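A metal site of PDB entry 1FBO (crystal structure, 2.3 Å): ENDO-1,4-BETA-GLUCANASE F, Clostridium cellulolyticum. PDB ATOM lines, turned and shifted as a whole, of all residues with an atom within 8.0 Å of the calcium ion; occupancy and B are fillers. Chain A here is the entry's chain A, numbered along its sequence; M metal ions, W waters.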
ATOM      1  N   GLN A 116     -14.934  18.620  24.037  1.00  0.00           N
ATOM      2  CA  GLN A 116     -15.203  20.038  23.815  1.00  0.00           C
ATOM      3  C   GLN A 116     -15.024  20.940  25.039  1.00  0.00           C
ATOM      4  O   GLN A 116     -15.385  22.115  25.011  1.00  0.00           O
ATOM      5  CB  GLN A 116     -16.611  20.228  23.240  1.00  0.00           C
ATOM      6  CG  GLN A 116     -16.754  19.833  21.772  1.00  0.00           C
ATOM      7  CD  GLN A 116     -16.431  18.373  21.504  1.00  0.00           C
ATOM      8  OE1 GLN A 116     -17.142  17.474  21.964  1.00  0.00           O
ATOM      9  NE2 GLN A 116     -15.359  18.136  20.764  1.00  0.00           N
ATOM     10  N   ASP A 117     -14.478  20.390  26.118  1.00  0.00           N
ATOM     11  CA  ASP A 117     -14.235  21.153  27.329  1.00  0.00           C
ATOM     12  C   ASP A 117     -13.043  20.544  28.072  1.00  0.00           C
ATOM     13  O   ASP A 117     -12.948  19.335  28.211  1.00  0.00           O
ATOM     14  CB  ASP A 117     -15.447  21.146  28.249  1.00  0.00           C
ATOM     15  CG  ASP A 117     -15.264  22.032  29.461  1.00  0.00           C
ATOM     16  OD1 ASP A 117     -15.007  23.249  29.277  1.00  0.00           O
ATOM     17  OD2 ASP A 117     -15.355  21.535  30.598  1.00  0.00           O
ATOM     18  N   PRO A 118     -12.128  21.389  28.558  1.00  0.00           N
ATOM     19  CA  PRO A 118     -10.949  20.911  29.275  1.00  0.00           C
ATOM     20  C   PRO A 118     -11.215  20.046  30.505  1.00  0.00           C
ATOM     21  O   PRO A 118     -10.393  19.204  30.856  1.00  0.00           O
ATOM     22  CB  PRO A 118     -10.214  22.195  29.621  1.00  0.00           C
ATOM     23  CG  PRO A 118     -10.566  23.094  28.479  1.00  0.00           C
ATOM     24  CD  PRO A 118     -12.041  22.847  28.334  1.00  0.00           C
ATOM     25  N   GLY A 183      -8.284  19.947  23.782  1.00  0.00           N
ATOM     26  CA  GLY A 183      -9.402  20.365  22.962  1.00  0.00           C
ATOM     27  C   GLY A 183      -9.612  21.803  22.528  1.00  0.00           C
ATOM     28  O   GLY A 183      -8.838  22.697  22.866  1.00  0.00           O
ATOM     29  N   GLU A 184     -10.692  22.015  21.776  1.00  0.00           N
ATOM     30  CA  GLU A 184     -11.049  23.311  21.209  1.00  0.00           C
ATOM     31  C   GLU A 184     -11.346  24.437  22.193  1.00  0.00           C
ATOM     32  O   GLU A 184     -11.285  25.597  21.831  1.00  0.00           O
ATOM     33  CB  GLU A 184     -12.238  23.157  20.263  1.00  0.00           C
ATOM     34  CG  GLU A 184     -13.563  22.859  20.956  1.00  0.00           C
ATOM     35  CD  GLU A 184     -14.747  22.859  19.993  1.00  0.00           C
ATOM     36  OE1 GLU A 184     -14.644  22.203  18.926  1.00  0.00           O
ATOM     37  OE2 GLU A 184     -15.782  23.492  20.298  1.00  0.00           O
ATOM     38  N   GLN A 185     -11.685  24.106  23.433  1.00  0.00           N
ATOM     39  CA  GLN A 185     -11.983  25.158  24.397  1.00  0.00           C
ATOM     40  C   GLN A 185     -10.805  25.521  25.279  1.00  0.00           C
ATOM     41  O   GLN A 185     -10.919  26.394  26.136  1.00  0.00           O
ATOM     42  CB  GLN A 185     -13.181  24.767  25.275  1.00  0.00           C
ATOM     43  CG  GLN A 185     -14.508  25.320  24.802  1.00  0.00           C
ATOM     44  CD  GLN A 185     -14.535  26.843  24.691  1.00  0.00           C
ATOM     45  OE1 GLN A 185     -13.951  27.551  25.525  1.00  0.00           O
ATOM     46  NE2 GLN A 185     -15.208  27.353  23.673  1.00  0.00           N
ATOM     47  N   GLU A 186      -9.668  24.867  25.071  1.00  0.00           N
ATOM     48  CA  GLU A 186      -8.487  25.183  25.882  1.00  0.00           C
ATOM     49  C   GLU A 186      -7.679  26.292  25.222  1.00  0.00           C
ATOM     50  O   GLU A 186      -6.850  26.028  24.350  1.00  0.00           O
ATOM     51  CB  GLU A 186      -7.601  23.949  26.064  1.00  0.00           C
ATOM     52  CG  GLU A 186      -6.386  24.222  26.925  1.00  0.00           C
ATOM     53  CD  GLU A 186      -5.500  23.013  27.090  1.00  0.00           C
ATOM     54  OE1 GLU A 186      -5.064  22.463  26.060  1.00  0.00           O
ATOM     55  OE2 GLU A 186      -5.237  22.609  28.237  1.00  0.00           O
ATOM     56  N   SER A 187      -7.929  27.525  25.633  1.00  0.00           N
ATOM     57  CA  SER A 187      -7.217  28.677  25.089  1.00  0.00           C
ATOM     58  C   SER A 187      -5.793  28.704  25.651  1.00  0.00           C
ATOM     59  O   SER A 187      -5.426  27.863  26.464  1.00  0.00           O
ATOM     60  CB  SER A 187      -7.933  29.971  25.467  1.00  0.00           C
ATOM     61  OG  SER A 187      -7.926  30.158  26.877  1.00  0.00           O
ATOM     62  N   THR A 188      -5.014  29.683  25.193  1.00  0.00           N
ATOM     63  CA  THR A 188      -3.644  29.865  25.647  1.00  0.00           C
ATOM     64  C   THR A 188      -3.619  30.128  27.151  1.00  0.00           C
ATOM     65  O   THR A 188      -2.619  29.865  27.807  1.00  0.00           O
ATOM     66  CB  THR A 188      -2.983  31.066  24.969  1.00  0.00           C
ATOM     67  OG1 THR A 188      -3.128  30.951  23.552  1.00  0.00           O
ATOM     68  CG2 THR A 188      -1.505  31.125  25.301  1.00  0.00           C
ATOM     69  N   TRP A 189      -4.723  30.645  27.675  1.00  0.00           N
ATOM     70  CA  TRP A 189      -4.850  30.962  29.087  1.00  0.00           C
ATOM     71  C   TRP A 189      -5.230  29.787  29.979  1.00  0.00           C
ATOM     72  O   TRP A 189      -5.123  29.876  31.197  1.00  0.00           O
ATOM     73  CB  TRP A 189      -5.909  32.051  29.300  1.00  0.00           C
ATOM     74  CG  TRP A 189      -5.679  33.250  28.480  1.00  0.00           C
ATOM     75  CD1 TRP A 189      -6.175  33.505  27.234  1.00  0.00           C
ATOM     76  CD2 TRP A 189      -4.866  34.381  28.821  1.00  0.00           C
ATOM     77  NE1 TRP A 189      -5.714  34.712  26.770  1.00  0.00           N
ATOM     78  CE2 TRP A 189      -4.899  35.268  27.733  1.00  0.00           C
ATOM     79  CE3 TRP A 189      -4.097  34.717  29.944  1.00  0.00           C
ATOM     80  CZ2 TRP A 189      -4.209  36.482  27.731  1.00  0.00           C
ATOM     81  CZ3 TRP A 189      -3.400  35.928  29.949  1.00  0.00           C
ATOM     82  CH2 TRP A 189      -3.472  36.794  28.843  1.00  0.00           C
ATOM     83  N   GLU A 190      -5.684  28.706  29.367  1.00  0.00           N
ATOM     84  CA  GLU A 190      -6.148  27.555  30.130  1.00  0.00           C
ATOM     85  C   GLU A 190      -5.280  26.306  30.069  1.00  0.00           C
ATOM     86  O   GLU A 190      -5.712  25.222  30.477  1.00  0.00           O
ATOM     87  CB  GLU A 190      -7.570  27.217  29.679  1.00  0.00           C
ATOM     88  CG  GLU A 190      -8.491  28.431  29.684  1.00  0.00           C
ATOM     89  CD  GLU A 190      -9.799  28.167  28.949  1.00  0.00           C
ATOM     90  OE1 GLU A 190     -10.613  27.361  29.438  1.00  0.00           O
ATOM     91  OE2 GLU A 190      -9.991  28.765  27.873  1.00  0.00           O
ATOM     92  N   ALA A 404     -11.831  27.196  19.354  1.00  0.00           N
ATOM     93  CA  ALA A 404     -13.027  28.034  19.414  1.00  0.00           C
ATOM     94  C   ALA A 404     -12.903  29.146  20.438  1.00  0.00           C
ATOM     95  O   ALA A 404     -13.839  29.910  20.652  1.00  0.00           O
ATOM     96  CB  ALA A 404     -14.263  27.160  19.748  1.00  0.00           C
ATOM     97  N   ASP A 405     -11.740  29.256  21.075  1.00  0.00           N
ATOM     98  CA  ASP A 405     -11.524  30.278  22.099  1.00  0.00           C
ATOM     99  C   ASP A 405     -10.167  30.983  21.963  1.00  0.00           C
ATOM    100  O   ASP A 405      -9.225  30.682  22.703  1.00  0.00           O
ATOM    101  CB  ASP A 405     -11.649  29.632  23.493  1.00  0.00           C
ATOM    102  CG  ASP A 405     -11.499  30.622  24.640  1.00  0.00           C
ATOM    103  OD1 ASP A 405     -11.422  31.847  24.399  1.00  0.00           O
ATOM    104  OD2 ASP A 405     -11.471  30.165  25.813  1.00  0.00           O
ATOM    105  N   PRO A 406     -10.054  31.950  21.023  1.00  0.00           N
ATOM    106  CA  PRO A 406     -11.075  32.424  20.091  1.00  0.00           C
ATOM    107  C   PRO A 406     -11.165  31.543  18.834  1.00  0.00           C
ATOM    108  O   PRO A 406     -10.289  30.722  18.592  1.00  0.00           O
ATOM    109  CB  PRO A 406     -10.590  33.831  19.761  1.00  0.00           C
ATOM    110  CG  PRO A 406      -9.104  33.622  19.669  1.00  0.00           C
ATOM    111  CD  PRO A 406      -8.831  32.768  20.912  1.00  0.00           C
ATOM    112  N   ARG A 549      -7.548  37.961  31.703  1.00  0.00           N
ATOM    113  CA  ARG A 549      -7.522  36.522  31.975  1.00  0.00           C
ATOM    114  C   ARG A 549      -6.241  36.115  32.715  1.00  0.00           C
ATOM    115  O   ARG A 549      -6.151  35.014  33.254  1.00  0.00           O
ATOM    116  CB  ARG A 549      -7.683  35.752  30.665  1.00  0.00           C
ATOM    117  CG  ARG A 549      -8.940  36.187  29.929  1.00  0.00           C
ATOM    118  CD  ARG A 549      -9.141  35.440  28.626  1.00  0.00           C
ATOM    119  NE  ARG A 549      -9.568  34.060  28.837  1.00  0.00           N
ATOM    120  CZ  ARG A 549      -9.973  33.255  27.868  1.00  0.00           C
ATOM    121  NH1 ARG A 549     -10.014  33.678  26.616  1.00  0.00           N
ATOM    122  NH2 ARG A 549     -10.351  32.008  28.156  1.00  0.00           N
ATOM    123  N   GLN A 553      -8.666  34.035  34.928  1.00  0.00           N
ATOM    124  CA  GLN A 553      -8.862  32.784  34.202  1.00  0.00           C
ATOM    125  C   GLN A 553      -8.451  31.577  35.044  1.00  0.00           C
ATOM    126  O   GLN A 553      -7.276  31.385  35.355  1.00  0.00           O
ATOM    127  CB  GLN A 553      -8.050  32.768  32.905  1.00  0.00           C
ATOM    128  CG  GLN A 553      -8.209  31.470  32.120  1.00  0.00           C
ATOM    129  CD  GLN A 553      -9.648  31.236  31.693  1.00  0.00           C
ATOM    130  OE1 GLN A 553     -10.156  31.920  30.806  1.00  0.00           O
ATOM    131  NE2 GLN A 553     -10.314  30.278  32.334  1.00  0.00           N
ATOM    132  N   GLU A 554      -9.438  30.762  35.401  1.00  0.00           N
ATOM    133  CA  GLU A 554      -9.158  29.575  36.188  1.00  0.00           C
ATOM    134  C   GLU A 554      -8.616  28.465  35.282  1.00  0.00           C
ATOM    135  O   GLU A 554      -9.051  28.318  34.135  1.00  0.00           O
ATOM    136  CB  GLU A 554     -10.440  29.105  36.887  1.00  0.00           C
ATOM    137  CG  GLU A 554     -10.210  28.006  37.915  1.00  0.00           C
ATOM    138  CD  GLU A 554     -11.499  27.508  38.548  1.00  0.00           C
ATOM    139  OE1 GLU A 554     -12.253  28.340  39.108  1.00  0.00           O
ATOM    140  OE2 GLU A 554     -11.746  26.280  38.494  1.00  0.00           O
HETATM  141 CA    CA M   1     -12.174  28.097  27.218  1.00  0.00          CA
HETATM  142  O   HOH W   1     -13.162  29.851  28.852  1.00  0.00           O
HETATM  143  O   HOH W   2     -13.520  26.564  28.628  1.00  0.00           O
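The side-chain carboxylate of Glu 190 sits close to the guanidinium group of Arg 549, 3.3 Å away.
The side-chain hydroxyl (OG) of Ser 187 sits close to the side-chain carboxylate (OE2) of Glu 190 (2.7 Å).
The side-chain carboxylate (OD1) of Asp 405 is in salt-bridge range of the guanidinium group (NH1) of Arg 549, 3.2 Å away.
The calcium ion is bound by OE2 of Glu 190, O of Gln 185, water W2, OE1 of Gln 185, water W1, OD2 of Asp 405 and OE1 of Glu 190.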
